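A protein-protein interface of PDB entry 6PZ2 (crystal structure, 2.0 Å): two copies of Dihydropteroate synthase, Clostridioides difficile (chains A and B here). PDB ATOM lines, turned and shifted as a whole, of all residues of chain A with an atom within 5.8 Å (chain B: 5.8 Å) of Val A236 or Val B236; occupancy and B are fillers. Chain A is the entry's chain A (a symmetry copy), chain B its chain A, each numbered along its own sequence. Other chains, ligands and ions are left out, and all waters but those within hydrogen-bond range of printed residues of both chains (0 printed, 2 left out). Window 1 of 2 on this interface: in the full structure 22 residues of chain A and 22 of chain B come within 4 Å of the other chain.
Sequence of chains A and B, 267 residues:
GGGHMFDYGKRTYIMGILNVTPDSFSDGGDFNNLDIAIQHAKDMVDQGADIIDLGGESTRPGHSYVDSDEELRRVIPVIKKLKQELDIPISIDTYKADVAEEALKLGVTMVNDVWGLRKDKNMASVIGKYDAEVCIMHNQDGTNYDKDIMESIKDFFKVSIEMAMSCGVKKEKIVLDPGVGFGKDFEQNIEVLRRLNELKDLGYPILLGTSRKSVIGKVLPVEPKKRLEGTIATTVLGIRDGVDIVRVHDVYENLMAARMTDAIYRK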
ATOM      1  N   GLU A 229     -17.947 -30.363   9.787  1.00  0.00           N
ATOM      2  CA  GLU A 229     -17.007 -29.250   9.663  1.00  0.00           C
ATOM      3  C   GLU A 229     -16.536 -28.850  11.064  1.00  0.00           C
ATOM      4  O   GLU A 229     -15.384 -28.442  11.204  1.00  0.00           O
ATOM      5  CB  GLU A 229     -17.367 -28.038   8.789  1.00  0.00           C
ATOM      6  CG  GLU A 229     -18.771 -27.821   8.304  1.00  0.00           C
ATOM      7  CD  GLU A 229     -19.438 -28.836   7.400  1.00  0.00           C
ATOM      8  OE1 GLU A 229     -18.929 -29.083   6.290  1.00  0.00           O
ATOM      9  OE2 GLU A 229     -20.489 -29.357   7.843  1.00  0.00           O
ATOM     10  N   THR A 231     -15.859 -31.099  13.384  1.00  0.00           N
ATOM     11  CA  THR A 231     -14.867 -32.100  13.678  1.00  0.00           C
ATOM     12  C   THR A 231     -13.572 -31.733  12.944  1.00  0.00           C
ATOM     13  O   THR A 231     -12.455 -31.797  13.499  1.00  0.00           O
ATOM     14  CB  THR A 231     -15.368 -33.474  13.220  1.00  0.00           C
ATOM     15  OG1 THR A 231     -16.564 -33.781  13.945  1.00  0.00           O
ATOM     16  CG2 THR A 231     -14.288 -34.525  13.336  1.00  0.00           C
ATOM     17  N   ILE A 232     -13.735 -31.322  11.690  1.00  0.00           N
ATOM     18  CA  ILE A 232     -12.549 -30.870  10.922  1.00  0.00           C
ATOM     19  C   ILE A 232     -11.874 -29.710  11.649  1.00  0.00           C
ATOM     20  O   ILE A 232     -10.659 -29.697  11.774  1.00  0.00           O
ATOM     21  CB  ILE A 232     -12.912 -30.536   9.466  1.00  0.00           C
ATOM     22  CG1 ILE A 232     -13.257 -31.829   8.724  1.00  0.00           C
ATOM     23  CG2 ILE A 232     -11.783 -29.780   8.780  1.00  0.00           C
ATOM     24  CD1 ILE A 232     -13.771 -31.569   7.341  1.00  0.00           C
ATOM     25  N   ALA A 233     -12.648 -28.811  12.254  1.00  0.00           N
ATOM     26  CA  ALA A 233     -12.022 -27.724  12.967  1.00  0.00           C
ATOM     27  C   ALA A 233     -11.167 -28.266  14.118  1.00  0.00           C
ATOM     28  O   ALA A 233     -10.016 -27.812  14.315  1.00  0.00           O
ATOM     29  CB  ALA A 233     -13.067 -26.755  13.467  1.00  0.00           C
ATOM     30  N   THR A 234     -11.700 -29.240  14.867  1.00  0.00           N
ATOM     31  CA  THR A 234     -10.947 -29.749  16.029  1.00  0.00           C
ATOM     32  C   THR A 234      -9.745 -30.593  15.570  1.00  0.00           C
ATOM     33  O   THR A 234      -8.695 -30.588  16.210  1.00  0.00           O
ATOM     34  CB  THR A 234     -11.854 -30.562  16.958  1.00  0.00           C
ATOM     35  OG1 THR A 234     -12.297 -31.711  16.243  1.00  0.00           O
ATOM     36  CG2 THR A 234     -13.065 -29.774  17.424  1.00  0.00           C
ATOM     37  N   THR A 235      -9.887 -31.309  14.473  1.00  0.00           N
ATOM     38  CA  THR A 235      -8.726 -32.006  13.908  1.00  0.00           C
ATOM     39  C   THR A 235      -7.603 -31.002  13.650  1.00  0.00           C
ATOM     40  O   THR A 235      -6.449 -31.229  14.001  1.00  0.00           O
ATOM     41  CB  THR A 235      -9.113 -32.746  12.628  1.00  0.00           C
ATOM     42  OG1 THR A 235      -9.882 -33.889  12.988  1.00  0.00           O
ATOM     43  CG2 THR A 235      -7.929 -33.209  11.803  1.00  0.00           C
ATOM     44  N   VAL A 236      -7.943 -29.890  13.027  1.00  0.00           N
ATOM     45  CA  VAL A 236      -6.942 -28.902  12.547  1.00  0.00           C
ATOM     46  C   VAL A 236      -6.243 -28.225  13.732  1.00  0.00           C
ATOM     47  O   VAL A 236      -5.010 -28.120  13.785  1.00  0.00           O
ATOM     48  CB  VAL A 236      -7.615 -27.880  11.602  1.00  0.00           C
ATOM     49  CG1 VAL A 236      -6.740 -26.679  11.275  1.00  0.00           C
ATOM     50  CG2 VAL A 236      -8.023 -28.568  10.316  1.00  0.00           C
ATOM     51  N   LEU A 237      -7.043 -27.777  14.687  1.00  0.00           N
ATOM     52  CA  LEU A 237      -6.541 -27.141  15.889  1.00  0.00           C
ATOM     53  C   LEU A 237      -5.723 -28.139  16.713  1.00  0.00           C
ATOM     54  O   LEU A 237      -4.692 -27.774  17.307  1.00  0.00           O
ATOM     55  CB  LEU A 237      -7.735 -26.602  16.700  1.00  0.00           C
ATOM     56  CG  LEU A 237      -8.523 -25.501  15.993  1.00  0.00           C
ATOM     57  CD1 LEU A 237      -9.825 -25.180  16.717  1.00  0.00           C
ATOM     58  CD2 LEU A 237      -7.688 -24.238  15.859  1.00  0.00           C
ATOM     59  N   GLY A 238      -6.215 -29.374  16.767  1.00  0.00           N
ATOM     60  CA  GLY A 238      -5.523 -30.413  17.497  1.00  0.00           C
ATOM     61  C   GLY A 238      -4.133 -30.607  16.943  1.00  0.00           C
ATOM     62  O   GLY A 238      -3.147 -30.603  17.684  1.00  0.00           O
ATOM     63  N   ILE A 239      -4.030 -30.742  15.639  1.00  0.00           N
ATOM     64  CA  ILE A 239      -2.701 -30.983  15.051  1.00  0.00           C
ATOM     65  C   ILE A 239      -1.797 -29.805  15.398  1.00  0.00           C
ATOM     66  O   ILE A 239      -0.677 -29.985  15.797  1.00  0.00           O
ATOM     67  CB  ILE A 239      -2.756 -31.141  13.529  1.00  0.00           C
ATOM     68  CG1 ILE A 239      -3.543 -32.394  13.144  1.00  0.00           C
ATOM     69  CG2 ILE A 239      -1.337 -31.144  12.948  1.00  0.00           C
ATOM     70  CD1 ILE A 239      -4.088 -32.356  11.728  1.00  0.00           C
ATOM     71  N   ARG A 240      -2.310 -28.585  15.324  1.00  0.00           N
ATOM     72  CA  ARG A 240      -1.470 -27.440  15.621  1.00  0.00           C
ATOM     73  C   ARG A 240      -0.997 -27.532  17.075  1.00  0.00           C
ATOM     74  O   ARG A 240       0.145 -27.176  17.360  1.00  0.00           O
ATOM     75  CB  ARG A 240      -2.201 -26.130  15.310  1.00  0.00           C
ATOM     76  CG  ARG A 240      -1.792 -24.965  16.195  1.00  0.00           C
ATOM     77  CD  ARG A 240      -1.271 -23.729  15.499  1.00  0.00           C
ATOM     78  NE  ARG A 240      -2.347 -22.781  15.380  1.00  0.00           N
ATOM     79  CZ  ARG A 240      -2.216 -21.474  15.197  1.00  0.00           C
ATOM     80  NH1 ARG A 240      -2.921 -20.904  14.235  1.00  0.00           N
ATOM     81  NH2 ARG A 240      -1.489 -20.735  16.011  1.00  0.00           N
ATOM     82  N   ASP A 241      -1.851 -28.040  17.967  1.00  0.00           N
ATOM     83  CA  ASP A 241      -1.536 -28.190  19.379  1.00  0.00           C
ATOM     84  C   ASP A 241      -0.693 -29.443  19.700  1.00  0.00           C
ATOM     85  O   ASP A 241      -0.384 -29.692  20.849  1.00  0.00           O
ATOM     86  CB  ASP A 241      -2.860 -28.208  20.146  1.00  0.00           C
ATOM     87  CG  ASP A 241      -3.459 -26.816  20.262  1.00  0.00           C
ATOM     88  OD1 ASP A 241      -2.656 -25.894  20.487  1.00  0.00           O
ATOM     89  OD2 ASP A 241      -4.710 -26.673  20.148  1.00  0.00           O
ATOM     90  N   ALA A 257      -7.835 -32.309   5.468  1.00  0.00           N
ATOM     91  CA  ALA A 257      -7.576 -31.178   6.357  1.00  0.00           C
ATOM     92  C   ALA A 257      -6.252 -31.344   7.120  1.00  0.00           C
ATOM     93  O   ALA A 257      -5.498 -30.368   7.372  1.00  0.00           O
ATOM     94  CB  ALA A 257      -8.758 -31.035   7.317  1.00  0.00           C
ATOM     95  N   ALA A 258      -5.975 -32.580   7.542  1.00  0.00           N
ATOM     96  CA  ALA A 258      -4.764 -32.865   8.277  1.00  0.00           C
ATOM     97  C   ALA A 258      -3.541 -32.629   7.382  1.00  0.00           C
ATOM     98  O   ALA A 258      -2.533 -32.153   7.852  1.00  0.00           O
ATOM     99  CB  ALA A 258      -4.780 -34.302   8.760  1.00  0.00           C
ATOM    100  N   THR A 261      -2.949 -28.931   7.238  1.00  0.00           N
ATOM    101  CA  THR A 261      -2.378 -28.461   8.477  1.00  0.00           C
ATOM    102  C   THR A 261      -0.928 -28.944   8.626  1.00  0.00           C
ATOM    103  O   THR A 261      -0.052 -28.195   9.085  1.00  0.00           O
ATOM    104  CB  THR A 261      -3.251 -28.911   9.658  1.00  0.00           C
ATOM    105  OG1 THR A 261      -4.635 -28.680   9.376  1.00  0.00           O
ATOM    106  CG2 THR A 261      -2.837 -28.214  10.924  1.00  0.00           C
ATOM    107  N   GLU B 229     -11.647 -28.989   2.048  1.00  0.00           N
ATOM    108  CA  GLU B 229     -11.233 -29.259   3.424  1.00  0.00           C
ATOM    109  C   GLU B 229      -9.907 -28.540   3.685  1.00  0.00           C
ATOM    110  O   GLU B 229      -9.689 -28.094   4.811  1.00  0.00           O
ATOM    111  CB  GLU B 229     -11.242 -30.701   3.957  1.00  0.00           C
ATOM    112  CG  GLU B 229     -11.369 -31.871   3.026  1.00  0.00           C
ATOM    113  CD  GLU B 229     -12.606 -32.042   2.170  1.00  0.00           C
ATOM    114  OE1 GLU B 229     -13.713 -32.167   2.726  1.00  0.00           O
ATOM    115  OE2 GLU B 229     -12.416 -32.057   0.931  1.00  0.00           O
ATOM    116  N   THR B 231      -9.316 -25.501   2.537  1.00  0.00           N
ATOM    117  CA  THR B 231      -9.737 -24.145   2.771  1.00  0.00           C
ATOM    118  C   THR B 231     -10.278 -24.042   4.203  1.00  0.00           C
ATOM    119  O   THR B 231      -9.978 -23.095   4.958  1.00  0.00           O
ATOM    120  CB  THR B 231     -10.823 -23.759   1.761  1.00  0.00           C
ATOM    121  OG1 THR B 231     -10.267 -23.850   0.445  1.00  0.00           O
ATOM    122  CG2 THR B 231     -11.428 -22.412   2.085  1.00  0.00           C
ATOM    123  N   ILE B 232     -11.067 -25.045   4.576  1.00  0.00           N
ATOM    124  CA  ILE B 232     -11.577 -25.077   5.969  1.00  0.00           C
ATOM    125  C   ILE B 232     -10.406 -25.087   6.948  1.00  0.00           C
ATOM    126  O   ILE B 232     -10.428 -24.357   7.927  1.00  0.00           O
ATOM    127  CB  ILE B 232     -12.552 -26.245   6.187  1.00  0.00           C
ATOM    128  CG1 ILE B 232     -13.845 -25.971   5.416  1.00  0.00           C
ATOM    129  CG2 ILE B 232     -12.821 -26.465   7.669  1.00  0.00           C
ATOM    130  CD1 ILE B 232     -14.786 -27.137   5.453  1.00  0.00           C
ATOM    131  N   ALA B 233      -9.324 -25.795   6.628  1.00  0.00           N
ATOM    132  CA  ALA B 233      -8.201 -25.792   7.533  1.00  0.00           C
ATOM    133  C   ALA B 233      -7.646 -24.371   7.686  1.00  0.00           C
ATOM    134  O   ALA B 233      -7.355 -23.928   8.822  1.00  0.00           O
ATOM    135  CB  ALA B 233      -7.137 -26.750   7.051  1.00  0.00           C
ATOM    136  N   THR B 234      -7.511 -23.646   6.569  1.00  0.00           N
ATOM    137  CA  THR B 234      -6.918 -22.298   6.652  1.00  0.00           C
ATOM    138  C   THR B 234      -7.894 -21.314   7.319  1.00  0.00           C
ATOM    139  O   THR B 234      -7.477 -20.405   8.035  1.00  0.00           O
ATOM    140  CB  THR B 234      -6.504 -21.793   5.266  1.00  0.00           C
ATOM    141  OG1 THR B 234      -7.685 -21.655   4.481  1.00  0.00           O
ATOM    142  CG2 THR B 234      -5.552 -22.741   4.562  1.00  0.00           C
ATOM    143  N   THR B 235      -9.182 -21.488   7.095  1.00  0.00           N
ATOM    144  CA  THR B 235     -10.160 -20.677   7.828  1.00  0.00           C
ATOM    145  C   THR B 235      -9.937 -20.843   9.331  1.00  0.00           C
ATOM    146  O   THR B 235      -9.898 -19.873  10.083  1.00  0.00           O
ATOM    147  CB  THR B 235     -11.584 -21.065   7.434  1.00  0.00           C
ATOM    148  OG1 THR B 235     -11.839 -20.560   6.126  1.00  0.00           O
ATOM    149  CG2 THR B 235     -12.650 -20.529   8.368  1.00  0.00           C
ATOM    150  N   VAL B 236      -9.796 -22.078   9.770  1.00  0.00           N
ATOM    151  CA  VAL B 236      -9.751 -22.416  11.217  1.00  0.00           C
ATOM    152  C   VAL B 236      -8.474 -21.862  11.859  1.00  0.00           C
ATOM    153  O   VAL B 236      -8.506 -21.219  12.917  1.00  0.00           O
ATOM    154  CB  VAL B 236      -9.890 -23.943  11.411  1.00  0.00           C
ATOM    155  CG1 VAL B 236      -9.588 -24.411  12.828  1.00  0.00           C
ATOM    156  CG2 VAL B 236     -11.289 -24.381  11.027  1.00  0.00           C
ATOM    157  N   LEU B 237      -7.352 -22.109  11.202  1.00  0.00           N
ATOM    158  CA  LEU B 237      -6.061 -21.629  11.657  1.00  0.00           C
ATOM    159  C   LEU B 237      -6.025 -20.099  11.624  1.00  0.00           C
ATOM    160  O   LEU B 237      -5.444 -19.460  12.520  1.00  0.00           O
ATOM    161  CB  LEU B 237      -4.964 -22.228  10.757  1.00  0.00           C
ATOM    162  CG  LEU B 237      -4.850 -23.749  10.841  1.00  0.00           C
ATOM    163  CD1 LEU B 237      -3.934 -24.311   9.760  1.00  0.00           C
ATOM    164  CD2 LEU B 237      -4.350 -24.180  12.210  1.00  0.00           C
ATOM    165  N   GLY B 238      -6.613 -19.536  10.571  1.00  0.00           N
ATOM    166  CA  GLY B 238      -6.663 -18.097  10.434  1.00  0.00           C
ATOM    167  C   GLY B 238      -7.378 -17.482  11.613  1.00  0.00           C
ATOM    168  O   GLY B 238      -6.872 -16.557  12.252  1.00  0.00           O
ATOM    169  N   ILE B 239      -8.539 -18.008  11.938  1.00  0.00           N
ATOM    170  CA  ILE B 239      -9.302 -17.413  13.050  1.00  0.00           C
ATOM    171  C   ILE B 239      -8.460 -17.504  14.318  1.00  0.00           C
ATOM    172  O   ILE B 239      -8.352 -16.559  15.054  1.00  0.00           O
ATOM    173  CB  ILE B 239     -10.639 -18.123  13.285  1.00  0.00           C
ATOM    174  CG1 ILE B 239     -11.567 -17.938  12.085  1.00  0.00           C
ATOM    175  CG2 ILE B 239     -11.273 -17.630  14.592  1.00  0.00           C
ATOM    176  CD1 ILE B 239     -12.655 -18.992  11.991  1.00  0.00           C
ATOM    177  N   ARG B 240      -7.787 -18.624  14.538  1.00  0.00           N
ATOM    178  CA  ARG B 240      -6.997 -18.755  15.749  1.00  0.00           C
ATOM    179  C   ARG B 240      -5.901 -17.685  15.746  1.00  0.00           C
ATOM    180  O   ARG B 240      -5.592 -17.138  16.803  1.00  0.00           O
ATOM    181  CB  ARG B 240      -6.448 -20.177  15.893  1.00  0.00           C
ATOM    182  CG  ARG B 240      -5.115 -20.257  16.618  1.00  0.00           C
ATOM    183  CD  ARG B 240      -5.059 -21.134  17.848  1.00  0.00           C
ATOM    184  NE  ARG B 240      -4.514 -22.413  17.476  1.00  0.00           N
ATOM    185  CZ  ARG B 240      -3.953 -23.289  18.298  1.00  0.00           C
ATOM    186  NH1 ARG B 240      -4.353 -24.547  18.238  1.00  0.00           N
ATOM    187  NH2 ARG B 240      -2.950 -22.950  19.084  1.00  0.00           N
ATOM    188  N   ASP B 241      -5.355 -17.369  14.569  1.00  0.00           N
ATOM    189  CA  ASP B 241      -4.308 -16.371  14.416  1.00  0.00           C
ATOM    190  C   ASP B 241      -4.831 -14.918  14.392  1.00  0.00           C
ATOM    191  O   ASP B 241      -4.055 -13.994  14.246  1.00  0.00           O
ATOM    192  CB  ASP B 241      -3.542 -16.701  13.133  1.00  0.00           C
ATOM    193  CG  ASP B 241      -2.610 -17.884  13.327  1.00  0.00           C
ATOM    194  OD1 ASP B 241      -1.998 -17.925  14.409  1.00  0.00           O
ATOM    195  OD2 ASP B 241      -2.488 -18.731  12.395  1.00  0.00           O
ATOM    196  N   ALA B 257     -17.384 -24.318  10.413  1.00  0.00           N
ATOM    197  CA  ALA B 257     -16.051 -24.458  10.996  1.00  0.00           C
ATOM    198  C   ALA B 257     -15.657 -23.222  11.821  1.00  0.00           C
ATOM    199  O   ALA B 257     -14.989 -23.312  12.883  1.00  0.00           O
ATOM    200  CB  ALA B 257     -15.052 -24.715   9.866  1.00  0.00           C
ATOM    201  N   ALA B 258     -16.025 -22.043  11.314  1.00  0.00           N
ATOM    202  CA  ALA B 258     -15.709 -20.806  11.992  1.00  0.00           C
ATOM    203  C   ALA B 258     -16.448 -20.742  13.334  1.00  0.00           C
ATOM    204  O   ALA B 258     -15.906 -20.251  14.298  1.00  0.00           O
ATOM    205  CB  ALA B 258     -16.107 -19.627  11.126  1.00  0.00           C
ATOM    206  N   THR B 261     -14.578 -22.905  15.755  1.00  0.00           N
ATOM    207  CA  THR B 261     -13.356 -22.260  16.174  1.00  0.00           C
ATOM    208  C   THR B 261     -13.659 -21.062  17.085  1.00  0.00           C
ATOM    209  O   THR B 261     -12.959 -20.829  18.083  1.00  0.00           O
ATOM    210  CB  THR B 261     -12.538 -21.844  14.942  1.00  0.00           C
ATOM    211  OG1 THR B 261     -12.493 -22.908  13.986  1.00  0.00           O
ATOM    212  CG2 THR B 261     -11.152 -21.419  15.341  1.00  0.00           C
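Of the printed residues of chain B, Glu A229 touches Ala B257. Val A236 touches just these residues of chain B: Ala B233, Val B236 and Leu B237. Of the printed residues of chain B, Ala A257 touches Glu B229 and Ala B233. Val B236 touches just these residues of chain A: Ala A233 (3.7 Å), Val A236 (3.96 Å) and Leu A237 (3.5 Å). Printed residues of chain A within 4 Å of Ala B257: Glu A229 and Ala A233. The nearest residue of chain B that does not touch Val A236 is Ile B232 (5.4 Å).
Ile A232 touches Ile B232 (CG2 to CG2, 3.6 Å). Ala A233 touches Val B236 (O to CG1, 3.7 Å). Ala A233 touches Ala B257. Ala A233 touches Thr B261 (CB to OG1, 3.9 Å). Ala B233 touches Val A236. Val A236 touches Val B236. Leu B237 touches Val A236. Leu A237 touches Val B236. Ala A257 touches Ala B233 (O to CB, 3.98 Å). Thr A261 touches Ala B233 (OG1 to CB, 3.9 Å).
Glu A229 touches Ala B257, and with the chains exchanged Ala A257 touches Glu B229. Ile B232 touches its own counterpart, Ile A232. Ala A233 touches Thr B261, and with the chains exchanged Thr A261 touches Ala B233. Val B236 touches its own counterpart, Val A236. 15 positions are printed for both chains. Of the 17 pairs that touch across the chains among the printed residues, 17 have their exchanged pair printed and touching as well.
Hydrophobic or aromatic side chains of chain A within 4 Å of the printed part of chain B: Ile A232, Ala A233, Val A236, Leu A237 and Ala A257. Of the 15 printed residues of chain B, 9 touch a printed residue of chain A. Hydrophobic or aromatic side chains of chain B within 4 Å of the printed part of chain A: Ile B232, Ala B233, Val B236, Leu B237 and Ala B257.
O of Ala B257 lies within hydrogen-bond range of OG1 of Thr B261, 2.8 Å away. O of Ala A257 lies within hydrogen-bond range of OG1 of Thr A261, 2.8 Å away.
The backbone carbonyl oxygen (O) of Leu B237 is in hydrogen-bond range of the guanidinium group (NH1) of Arg A240 (3.4 Å). The guanidinium group (NH1) of Arg B240 is in hydrogen-bond range of the backbone carbonyl oxygen (O) of Leu A237, 3.4 Å away. The guanidinium group (NH1) of Arg B240 lies within salt-bridge range of the side-chain carboxylate (OD2) of Asp A241 (2.9 Å). The side-chain carboxylate (OD2) of Asp B241 is in salt-bridge range of the guanidinium group (NH1) of Arg A240 (2.9 Å). NE of Arg A240 lies close to NE of Arg B240.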
